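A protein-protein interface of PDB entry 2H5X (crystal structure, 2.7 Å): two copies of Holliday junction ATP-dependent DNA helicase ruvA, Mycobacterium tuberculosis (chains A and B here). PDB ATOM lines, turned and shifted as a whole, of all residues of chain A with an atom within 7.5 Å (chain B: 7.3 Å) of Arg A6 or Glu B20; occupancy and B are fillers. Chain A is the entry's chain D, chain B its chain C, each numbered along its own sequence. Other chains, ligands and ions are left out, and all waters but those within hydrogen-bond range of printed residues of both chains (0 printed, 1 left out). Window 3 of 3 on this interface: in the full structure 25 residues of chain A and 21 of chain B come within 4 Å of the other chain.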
ATOM      1  N   SER A   4     -22.494 -15.655  -1.577  1.00  0.00           N
ATOM      2  CA  SER A   4     -22.690 -15.624  -3.020  1.00  0.00           C
ATOM      3  C   SER A   4     -21.694 -16.515  -3.762  1.00  0.00           C
ATOM      4  O   SER A   4     -20.623 -16.849  -3.250  1.00  0.00           O
ATOM      5  CB  SER A   4     -22.597 -14.180  -3.553  1.00  0.00           C
ATOM      6  OG  SER A   4     -21.249 -13.765  -3.725  1.00  0.00           O
ATOM      7  N   VAL A   5     -22.073 -16.897  -4.978  1.00  0.00           N
ATOM      8  CA  VAL A   5     -21.251 -17.736  -5.835  1.00  0.00           C
ATOM      9  C   VAL A   5     -21.231 -17.164  -7.262  1.00  0.00           C
ATOM     10  O   VAL A   5     -22.280 -16.934  -7.860  1.00  0.00           O
ATOM     11  CB  VAL A   5     -21.787 -19.186  -5.852  1.00  0.00           C
ATOM     12  CG1 VAL A   5     -20.954 -20.044  -6.786  1.00  0.00           C
ATOM     13  CG2 VAL A   5     -21.745 -19.770  -4.444  1.00  0.00           C
ATOM     14  N   ARG A   6     -20.034 -16.932  -7.798  1.00  0.00           N
ATOM     15  CA  ARG A   6     -19.878 -16.392  -9.146  1.00  0.00           C
ATOM     16  C   ARG A   6     -18.951 -17.282  -9.979  1.00  0.00           C
ATOM     17  O   ARG A   6     -17.782 -17.478  -9.644  1.00  0.00           O
ATOM     18  CB  ARG A   6     -19.302 -14.981  -9.071  1.00  0.00           C
ATOM     19  CG  ARG A   6     -19.375 -14.192 -10.358  1.00  0.00           C
ATOM     20  CD  ARG A   6     -18.369 -13.071 -10.305  1.00  0.00           C
ATOM     21  NE  ARG A   6     -17.047 -13.630 -10.056  1.00  0.00           N
ATOM     22  CZ  ARG A   6     -15.925 -12.928 -10.006  1.00  0.00           C
ATOM     23  NH1 ARG A   6     -15.960 -11.618 -10.191  1.00  0.00           N
ATOM     24  NH2 ARG A   6     -14.767 -13.536  -9.769  1.00  0.00           N
ATOM     25  N   GLY A   7     -19.470 -17.826 -11.068  1.00  0.00           N
ATOM     26  CA  GLY A   7     -18.645 -18.681 -11.894  1.00  0.00           C
ATOM     27  C   GLY A   7     -19.345 -19.129 -13.154  1.00  0.00           C
ATOM     28  O   GLY A   7     -20.313 -18.515 -13.604  1.00  0.00           O
ATOM     29  N   GLU A   8     -18.851 -20.212 -13.731  1.00  0.00           N
ATOM     30  CA  GLU A   8     -19.427 -20.738 -14.952  1.00  0.00           C
ATOM     31  C   GLU A   8     -20.606 -21.631 -14.624  1.00  0.00           C
ATOM     32  O   GLU A   8     -20.514 -22.505 -13.764  1.00  0.00           O
ATOM     33  CB  GLU A   8     -18.370 -21.537 -15.718  1.00  0.00           C
ATOM     34  CG  GLU A   8     -18.803 -22.037 -17.083  1.00  0.00           C
ATOM     35  CD  GLU A   8     -17.751 -22.932 -17.722  1.00  0.00           C
ATOM     36  OE1 GLU A   8     -16.569 -22.529 -17.762  1.00  0.00           O
ATOM     37  OE2 GLU A   8     -18.106 -24.039 -18.185  1.00  0.00           O
ATOM     38  N   VAL A   9     -21.722 -21.402 -15.297  1.00  0.00           N
ATOM     39  CA  VAL A   9     -22.890 -22.233 -15.074  1.00  0.00           C
ATOM     40  C   VAL A   9     -22.584 -23.558 -15.746  1.00  0.00           C
ATOM     41  O   VAL A   9     -22.526 -23.628 -16.960  1.00  0.00           O
ATOM     42  CB  VAL A   9     -24.139 -21.632 -15.728  1.00  0.00           C
ATOM     43  CG1 VAL A   9     -25.298 -22.590 -15.612  1.00  0.00           C
ATOM     44  CG2 VAL A   9     -24.465 -20.304 -15.078  1.00  0.00           C
ATOM     45  N   ILE A  19     -22.830 -23.870 -10.304  1.00  0.00           N
ATOM     46  CA  ILE A  19     -21.915 -22.825 -10.730  1.00  0.00           C
ATOM     47  C   ILE A  19     -20.526 -23.234 -10.282  1.00  0.00           C
ATOM     48  O   ILE A  19     -20.322 -23.572  -9.115  1.00  0.00           O
ATOM     49  CB  ILE A  19     -22.266 -21.469 -10.080  1.00  0.00           C
ATOM     50  CG1 ILE A  19     -23.682 -21.046 -10.485  1.00  0.00           C
ATOM     51  CG2 ILE A  19     -21.224 -20.427 -10.459  1.00  0.00           C
ATOM     52  CD1 ILE A  19     -24.140 -19.771  -9.816  1.00  0.00           C
ATOM     53  N   GLU A  20     -19.574 -23.204 -11.208  1.00  0.00           N
ATOM     54  CA  GLU A  20     -18.202 -23.581 -10.892  1.00  0.00           C
ATOM     55  C   GLU A  20     -17.354 -22.356 -10.575  1.00  0.00           C
ATOM     56  O   GLU A  20     -17.262 -21.425 -11.373  1.00  0.00           O
ATOM     57  CB  GLU A  20     -17.571 -24.358 -12.050  1.00  0.00           C
ATOM     58  CG  GLU A  20     -16.199 -24.923 -11.722  1.00  0.00           C
ATOM     59  CD  GLU A  20     -15.498 -25.512 -12.928  1.00  0.00           C
ATOM     60  OE1 GLU A  20     -15.976 -26.525 -13.483  1.00  0.00           O
ATOM     61  OE2 GLU A  20     -14.460 -24.950 -13.327  1.00  0.00           O
ATOM     62  N   ALA A  21     -16.748 -22.369  -9.397  1.00  0.00           N
ATOM     63  CA  ALA A  21     -15.898 -21.285  -8.948  1.00  0.00           C
ATOM     64  C   ALA A  21     -14.639 -21.926  -8.397  1.00  0.00           C
ATOM     65  O   ALA A  21     -14.693 -22.657  -7.403  1.00  0.00           O
ATOM     66  CB  ALA A  21     -16.593 -20.482  -7.866  1.00  0.00           C
ATOM     67  N   ALA A  22     -13.512 -21.653  -9.050  1.00  0.00           N
ATOM     68  CA  ALA A  22     -12.230 -22.202  -8.640  1.00  0.00           C
ATOM     69  C   ALA A  22     -12.263 -23.720  -8.754  1.00  0.00           C
ATOM     70  O   ALA A  22     -11.786 -24.435  -7.873  1.00  0.00           O
ATOM     71  CB  ALA A  22     -11.903 -21.783  -7.208  1.00  0.00           C
ATOM     72  N   VAL A  24     -14.521 -25.620  -8.264  1.00  0.00           N
ATOM     73  CA  VAL A  24     -15.469 -26.219  -7.333  1.00  0.00           C
ATOM     74  C   VAL A  24     -16.864 -25.849  -7.819  1.00  0.00           C
ATOM     75  O   VAL A  24     -17.200 -24.666  -7.930  1.00  0.00           O
ATOM     76  CB  VAL A  24     -15.279 -25.679  -5.899  1.00  0.00           C
ATOM     77  CG1 VAL A  24     -16.316 -26.281  -4.972  1.00  0.00           C
ATOM     78  CG2 VAL A  24     -13.881 -25.996  -5.407  1.00  0.00           C
ATOM     79  N   TYR A  26     -20.640 -25.614  -7.110  1.00  0.00           N
ATOM     80  CA  TYR A  26     -21.601 -25.583  -6.016  1.00  0.00           C
ATOM     81  C   TYR A  26     -23.041 -25.761  -6.504  1.00  0.00           C
ATOM     82  O   TYR A  26     -23.453 -25.159  -7.496  1.00  0.00           O
ATOM     83  CB  TYR A  26     -21.492 -24.257  -5.254  1.00  0.00           C
ATOM     84  CG  TYR A  26     -20.135 -23.981  -4.659  1.00  0.00           C
ATOM     85  CD1 TYR A  26     -19.103 -23.468  -5.438  1.00  0.00           C
ATOM     86  CD2 TYR A  26     -19.874 -24.252  -3.312  1.00  0.00           C
ATOM     87  CE1 TYR A  26     -17.840 -23.230  -4.897  1.00  0.00           C
ATOM     88  CE2 TYR A  26     -18.613 -24.023  -2.759  1.00  0.00           C
ATOM     89  CZ  TYR A  26     -17.603 -23.511  -3.558  1.00  0.00           C
ATOM     90  OH  TYR A  26     -16.349 -23.294  -3.029  1.00  0.00           O
ATOM     91  N   GLU A  43     -20.987 -17.137 -17.525  1.00  0.00           N
ATOM     92  CA  GLU A  43     -20.564 -16.714 -16.198  1.00  0.00           C
ATOM     93  C   GLU A  43     -21.783 -16.128 -15.487  1.00  0.00           C
ATOM     94  O   GLU A  43     -22.525 -15.336 -16.071  1.00  0.00           O
ATOM     95  CB  GLU A  43     -19.456 -15.661 -16.299  1.00  0.00           C
ATOM     96  CG  GLU A  43     -18.335 -15.832 -15.276  1.00  0.00           C
ATOM     97  CD  GLU A  43     -17.457 -17.048 -15.563  1.00  0.00           C
ATOM     98  OE1 GLU A  43     -17.992 -18.174 -15.638  1.00  0.00           O
ATOM     99  OE2 GLU A  43     -16.227 -16.879 -15.713  1.00  0.00           O
ATOM    100  N   ALA A  44     -21.998 -16.531 -14.235  1.00  0.00           N
ATOM    101  CA  ALA A  44     -23.130 -16.029 -13.461  1.00  0.00           C
ATOM    102  C   ALA A  44     -22.859 -15.950 -11.959  1.00  0.00           C
ATOM    103  O   ALA A  44     -21.938 -16.597 -11.449  1.00  0.00           O
ATOM    104  CB  ALA A  44     -24.332 -16.893 -13.707  1.00  0.00           C
ATOM    105  N   ARG A  45     -23.662 -15.145 -11.261  1.00  0.00           N
ATOM    106  CA  ARG A  45     -23.534 -14.988  -9.815  1.00  0.00           C
ATOM    107  C   ARG A  45     -24.890 -14.964  -9.108  1.00  0.00           C
ATOM    108  O   ARG A  45     -25.793 -14.244  -9.507  1.00  0.00           O
ATOM    109  CB  ARG A  45     -22.784 -13.708  -9.487  1.00  0.00           C
ATOM    110  CG  ARG A  45     -22.392 -13.618  -8.034  1.00  0.00           C
ATOM    111  CD  ARG A  45     -21.639 -12.338  -7.770  1.00  0.00           C
ATOM    112  NE  ARG A  45     -22.528 -11.181  -7.740  1.00  0.00           N
ATOM    113  CZ  ARG A  45     -22.106  -9.923  -7.782  1.00  0.00           C
ATOM    114  NH1 ARG A  45     -20.804  -9.663  -7.866  1.00  0.00           N
ATOM    115  NH2 ARG A  45     -22.984  -8.927  -7.724  1.00  0.00           N
ATOM    116  N   LEU A  46     -25.041 -15.759  -8.059  1.00  0.00           N
ATOM    117  CA  LEU A  46     -26.303 -15.772  -7.332  1.00  0.00           C
ATOM    118  C   LEU A  46     -26.123 -15.421  -5.869  1.00  0.00           C
ATOM    119  O   LEU A  46     -25.215 -15.925  -5.211  1.00  0.00           O
ATOM    120  CB  LEU A  46     -26.979 -17.143  -7.419  1.00  0.00           C
ATOM    121  CG  LEU A  46     -27.723 -17.557  -8.688  1.00  0.00           C
ATOM    122  CD1 LEU A  46     -28.502 -18.841  -8.404  1.00  0.00           C
ATOM    123  CD2 LEU A  46     -28.666 -16.456  -9.124  1.00  0.00           C
ATOM    124  N   VAL B   5      -9.906 -13.883   5.154  1.00  0.00           N
ATOM    125  CA  VAL B   5     -10.535 -13.751   3.843  1.00  0.00           C
ATOM    126  C   VAL B   5     -10.039 -12.480   3.138  1.00  0.00           C
ATOM    127  O   VAL B   5     -10.141 -11.378   3.687  1.00  0.00           O
ATOM    128  CB  VAL B   5     -12.087 -13.696   3.971  1.00  0.00           C
ATOM    129  CG1 VAL B   5     -12.712 -13.426   2.616  1.00  0.00           C
ATOM    130  CG2 VAL B   5     -12.619 -15.014   4.513  1.00  0.00           C
ATOM    131  N   ARG B   6      -9.507 -12.646   1.923  1.00  0.00           N
ATOM    132  CA  ARG B   6      -8.975 -11.538   1.124  1.00  0.00           C
ATOM    133  C   ARG B   6      -9.529 -11.580  -0.301  1.00  0.00           C
ATOM    134  O   ARG B   6      -9.295 -12.531  -1.043  1.00  0.00           O
ATOM    135  CB  ARG B   6      -7.452 -11.627   1.069  1.00  0.00           C
ATOM    136  CG  ARG B   6      -6.757 -10.430   0.452  1.00  0.00           C
ATOM    137  CD  ARG B   6      -5.372 -10.815  -0.053  1.00  0.00           C
ATOM    138  NE  ARG B   6      -5.460 -11.624  -1.268  1.00  0.00           N
ATOM    139  CZ  ARG B   6      -4.502 -12.430  -1.718  1.00  0.00           C
ATOM    140  NH1 ARG B   6      -3.355 -12.547  -1.056  1.00  0.00           N
ATOM    141  NH2 ARG B   6      -4.704 -13.139  -2.828  1.00  0.00           N
ATOM    142  N   GLY B   7     -10.262 -10.542  -0.685  1.00  0.00           N
ATOM    143  CA  GLY B   7     -10.835 -10.495  -2.015  1.00  0.00           C
ATOM    144  C   GLY B   7     -11.463  -9.140  -2.265  1.00  0.00           C
ATOM    145  O   GLY B   7     -11.167  -8.181  -1.544  1.00  0.00           O
ATOM    146  N   GLU B   8     -12.325  -9.061  -3.279  1.00  0.00           N
ATOM    147  CA  GLU B   8     -13.004  -7.816  -3.624  1.00  0.00           C
ATOM    148  C   GLU B   8     -14.173  -7.606  -2.685  1.00  0.00           C
ATOM    149  O   GLU B   8     -14.923  -8.539  -2.398  1.00  0.00           O
ATOM    150  CB  GLU B   8     -13.537  -7.863  -5.056  1.00  0.00           C
ATOM    151  CG  GLU B   8     -14.059  -6.527  -5.549  1.00  0.00           C
ATOM    152  CD  GLU B   8     -14.965  -6.652  -6.765  1.00  0.00           C
ATOM    153  OE1 GLU B   8     -14.623  -7.410  -7.697  1.00  0.00           O
ATOM    154  OE2 GLU B   8     -16.022  -5.982  -6.793  1.00  0.00           O
ATOM    155  N   VAL B   9     -14.332  -6.379  -2.200  1.00  0.00           N
ATOM    156  CA  VAL B   9     -15.442  -6.076  -1.311  1.00  0.00           C
ATOM    157  C   VAL B   9     -16.670  -5.858  -2.182  1.00  0.00           C
ATOM    158  O   VAL B   9     -16.700  -4.948  -3.005  1.00  0.00           O
ATOM    159  CB  VAL B   9     -15.157  -4.819  -0.478  1.00  0.00           C
ATOM    160  CG1 VAL B   9     -16.325  -4.544   0.461  1.00  0.00           C
ATOM    161  CG2 VAL B   9     -13.866  -5.010   0.308  1.00  0.00           C
ATOM    162  N   LEU B  10     -17.679  -6.701  -2.006  1.00  0.00           N
ATOM    163  CA  LEU B  10     -18.891  -6.608  -2.810  1.00  0.00           C
ATOM    164  C   LEU B  10     -19.993  -5.757  -2.161  1.00  0.00           C
ATOM    165  O   LEU B  10     -20.837  -5.176  -2.850  1.00  0.00           O
ATOM    166  CB  LEU B  10     -19.437  -8.017  -3.097  1.00  0.00           C
ATOM    167  CG  LEU B  10     -18.545  -9.070  -3.769  1.00  0.00           C
ATOM    168  CD1 LEU B  10     -19.284 -10.399  -3.791  1.00  0.00           C
ATOM    169  CD2 LEU B  10     -18.163  -8.650  -5.173  1.00  0.00           C
ATOM    170  N   GLU B  11     -19.979  -5.696  -0.835  1.00  0.00           N
ATOM    171  CA  GLU B  11     -20.967  -4.931  -0.086  1.00  0.00           C
ATOM    172  C   GLU B  11     -20.437  -4.608   1.304  1.00  0.00           C
ATOM    173  O   GLU B  11     -19.761  -5.422   1.927  1.00  0.00           O
ATOM    174  CB  GLU B  11     -22.261  -5.735   0.034  1.00  0.00           C
ATOM    175  CG  GLU B  11     -23.324  -5.090   0.908  1.00  0.00           C
ATOM    176  CD  GLU B  11     -24.560  -5.962   1.063  1.00  0.00           C
ATOM    177  OE1 GLU B  11     -24.441  -7.078   1.619  1.00  0.00           O
ATOM    178  OE2 GLU B  11     -25.651  -5.533   0.627  1.00  0.00           O
ATOM    179  N   VAL B  18     -19.054  -8.253   2.834  1.00  0.00           N
ATOM    180  CA  VAL B  18     -18.998  -9.448   2.000  1.00  0.00           C
ATOM    181  C   VAL B  18     -17.748  -9.364   1.131  1.00  0.00           C
ATOM    182  O   VAL B  18     -17.637  -8.483   0.278  1.00  0.00           O
ATOM    183  CB  VAL B  18     -20.235  -9.571   1.073  1.00  0.00           C
ATOM    184  CG1 VAL B  18     -20.152 -10.852   0.242  1.00  0.00           C
ATOM    185  CG2 VAL B  18     -21.490  -9.580   1.893  1.00  0.00           C
ATOM    186  N   ILE B  19     -16.809 -10.273   1.356  1.00  0.00           N
ATOM    187  CA  ILE B  19     -15.576 -10.290   0.581  1.00  0.00           C
ATOM    188  C   ILE B  19     -15.635 -11.460  -0.399  1.00  0.00           C
ATOM    189  O   ILE B  19     -15.821 -12.601   0.015  1.00  0.00           O
ATOM    190  CB  ILE B  19     -14.337 -10.487   1.488  1.00  0.00           C
ATOM    191  CG1 ILE B  19     -14.449  -9.626   2.748  1.00  0.00           C
ATOM    192  CG2 ILE B  19     -13.077 -10.129   0.728  1.00  0.00           C
ATOM    193  CD1 ILE B  19     -14.612  -8.167   2.478  1.00  0.00           C
ATOM    194  N   GLU B  20     -15.495 -11.187  -1.693  1.00  0.00           N
ATOM    195  CA  GLU B  20     -15.541 -12.265  -2.670  1.00  0.00           C
ATOM    196  C   GLU B  20     -14.129 -12.791  -2.902  1.00  0.00           C
ATOM    197  O   GLU B  20     -13.283 -12.100  -3.475  1.00  0.00           O
ATOM    198  CB  GLU B  20     -16.157 -11.786  -3.987  1.00  0.00           C
ATOM    199  CG  GLU B  20     -16.290 -12.888  -5.019  1.00  0.00           C
ATOM    200  CD  GLU B  20     -16.926 -12.429  -6.321  1.00  0.00           C
ATOM    201  OE1 GLU B  20     -18.166 -12.279  -6.380  1.00  0.00           O
ATOM    202  OE2 GLU B  20     -16.178 -12.220  -7.294  1.00  0.00           O
ATOM    203  N   ALA B  21     -13.878 -14.009  -2.424  1.00  0.00           N
ATOM    204  CA  ALA B  21     -12.579 -14.651  -2.572  1.00  0.00           C
ATOM    205  C   ALA B  21     -12.665 -15.807  -3.560  1.00  0.00           C
ATOM    206  O   ALA B  21     -13.233 -16.854  -3.257  1.00  0.00           O
ATOM    207  CB  ALA B  21     -12.092 -15.156  -1.216  1.00  0.00           C
ATOM    208  N   ALA B  22     -12.106 -15.608  -4.748  1.00  0.00           N
ATOM    209  CA  ALA B  22     -12.112 -16.638  -5.780  1.00  0.00           C
ATOM    210  C   ALA B  22     -13.527 -17.020  -6.215  1.00  0.00           C
ATOM    211  O   ALA B  22     -13.849 -18.202  -6.360  1.00  0.00           O
ATOM    212  CB  ALA B  22     -11.364 -17.874  -5.288  1.00  0.00           C
ATOM    213  N   GLY B  23     -14.371 -16.011  -6.411  1.00  0.00           N
ATOM    214  CA  GLY B  23     -15.730 -16.264  -6.853  1.00  0.00           C
ATOM    215  C   GLY B  23     -16.737 -16.526  -5.752  1.00  0.00           C
ATOM    216  O   GLY B  23     -17.946 -16.424  -5.976  1.00  0.00           O
ATOM    217  N   VAL B  24     -16.254 -16.871  -4.562  1.00  0.00           N
ATOM    218  CA  VAL B  24     -17.154 -17.138  -3.455  1.00  0.00           C
ATOM    219  C   VAL B  24     -17.161 -15.940  -2.518  1.00  0.00           C
ATOM    220  O   VAL B  24     -16.110 -15.513  -2.032  1.00  0.00           O
ATOM    221  CB  VAL B  24     -16.735 -18.412  -2.684  1.00  0.00           C
ATOM    222  CG1 VAL B  24     -17.712 -18.683  -1.545  1.00  0.00           C
ATOM    223  CG2 VAL B  24     -16.694 -19.591  -3.635  1.00  0.00           C
ATOM    224  N   GLY B  25     -18.354 -15.393  -2.285  1.00  0.00           N
ATOM    225  CA  GLY B  25     -18.495 -14.243  -1.414  1.00  0.00           C
ATOM    226  C   GLY B  25     -18.824 -14.643   0.006  1.00  0.00           C
ATOM    227  O   GLY B  25     -19.902 -15.180   0.295  1.00  0.00           O
ATOM    228  N   TYR B  26     -17.890 -14.383   0.910  1.00  0.00           N
ATOM    229  CA  TYR B  26     -18.113 -14.732   2.301  1.00  0.00           C
ATOM    230  C   TYR B  26     -18.634 -13.562   3.125  1.00  0.00           C
ATOM    231  O   TYR B  26     -18.149 -12.429   3.028  1.00  0.00           O
ATOM    232  CB  TYR B  26     -16.828 -15.274   2.926  1.00  0.00           C
ATOM    233  CG  TYR B  26     -16.213 -16.427   2.170  1.00  0.00           C
ATOM    234  CD1 TYR B  26     -15.482 -16.206   1.006  1.00  0.00           C
ATOM    235  CD2 TYR B  26     -16.317 -17.732   2.649  1.00  0.00           C
ATOM    236  CE1 TYR B  26     -14.858 -17.250   0.344  1.00  0.00           C
ATOM    237  CE2 TYR B  26     -15.700 -18.793   1.993  1.00  0.00           C
ATOM    238  CZ  TYR B  26     -14.968 -18.547   0.844  1.00  0.00           C
ATOM    239  OH  TYR B  26     -14.331 -19.591   0.199  1.00  0.00           O
ATOM    240  N   GLU B  43      -9.932  -4.234  -2.980  1.00  0.00           N
ATOM    241  CA  GLU B  43      -9.329  -5.448  -2.437  1.00  0.00           C
ATOM    242  C   GLU B  43      -9.179  -5.255  -0.927  1.00  0.00           C
ATOM    243  O   GLU B  43      -8.763  -4.191  -0.472  1.00  0.00           O
ATOM    244  CB  GLU B  43      -7.940  -5.675  -3.046  1.00  0.00           C
ATOM    245  CG  GLU B  43      -7.352  -7.043  -2.767  1.00  0.00           C
ATOM    246  CD  GLU B  43      -7.963  -8.108  -3.654  1.00  0.00           C
ATOM    247  OE1 GLU B  43      -9.092  -7.900  -4.155  1.00  0.00           O
ATOM    248  OE2 GLU B  43      -7.324  -9.161  -3.849  1.00  0.00           O
ATOM    249  N   ALA B  44      -9.510  -6.272  -0.143  1.00  0.00           N
ATOM    250  CA  ALA B  44      -9.379  -6.148   1.303  1.00  0.00           C
ATOM    251  C   ALA B  44      -9.154  -7.496   1.971  1.00  0.00           C
ATOM    252  O   ALA B  44      -9.628  -8.524   1.483  1.00  0.00           O
ATOM    253  CB  ALA B  44     -10.628  -5.482   1.888  1.00  0.00           C
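NH1 of Arg A6 lies within salt-bridge range of OE2 of Glu B20, at 3.0 Å.
The backbone NH (N) of Arg A6 sits at hydrogen-bond distance from the backbone carbonyl oxygen (O) of Gly B23.
O of Ser A4 sits at hydrogen-bond distance from N of Gly B25, 2.9 Å away.
The backbone NH of Glu B20 sits at hydrogen-bond distance from the backbone carbonyl oxygen of Glu B8 (2.8 Å).
O of Val B18 sits at hydrogen-bond distance from N of Leu B10 (2.9 Å).
N of Leu A46 is in hydrogen-bond range of O of Val A5 (3.0 Å).
The backbone NH (N) of Tyr A26 sits at hydrogen-bond distance from the backbone carbonyl oxygen (O) of Ile A19, at 2.9 Å.
Among the printed residues, merely in contact across the chains: Ser A4 with Leu B10 (3.9 Å), Ser A4 with Gly B23 (3.8 Å), Ser A4 with Val B24 (3.5 Å), Val A5 with Gly B23 (3.6 Å), Ala A21 with Ala B22 (3.9 Å), Tyr A26 with Val B24 (3.8 Å), Arg A45 with Leu B10 (3.9 Å) and Arg A45 with Glu B20 (3.7 Å).
Printed residues of chain B within 4 Å of Ser A4: Leu B10 (3.9 Å), Gly B23 (3.8 Å), Val B24 (3.5 Å) and Gly B25 (2.9 Å).
Of chain B, only Glu B20 and Gly B23 come within 4 Å of Arg A6.
Of chain A, only Arg A6 and Arg A45 come within 4 Å of Glu B20.
Of the printed residues of chain A, Gly B25 touches Ser A4.
The nearest residue of chain A that does not touch Glu B20 is Ser A4 (4.3 Å).
The nearest printed residue of chain A that does not touch Gly B25 is Val A5 (4.8 Å).
Of the 16 printed residues of chain A, 6 touch a printed residue of chain B.
Printed residues of chain A that touch a printed residue of chain B: Ser A4, Val A5, Arg A6, Ala A21, Tyr A26 and Arg A45.
Hydrophobic or aromatic side chains of chain A that line the printed part of chain B: Ala A21 and Tyr A26.
Of the 18 printed residues of chain B, 6 touch a printed residue of chain A.
Hydrophobic or aromatic side chains of chain B that line the printed part of chain A: Leu B10 and Val B24.
Among the printed residues, 11 pairs touch across the chains.
Among the printed residues, Asp or Glu carboxylates within 4 Å of a Lys or Arg side-chain nitrogen of the other chain: Arg A6 with Glu B20 (3.0 Å).
Arg A6 touches Glu B20, but with the chains exchanged Glu A20 does not touch Arg B6 (15.8 Å).
Ala A21 touches Ala B22, but with the chains exchanged Ala A22 does not touch Ala B21 (6.5 Å).
Tyr A26 touches Val B24, but with the chains exchanged Val A24 does not touch Tyr B26 (8.5 Å).
Positions printed for both chains: 5, 6, 7, 8, 9, 19, 20, 21, 22, 24, 26, 43 and 44.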
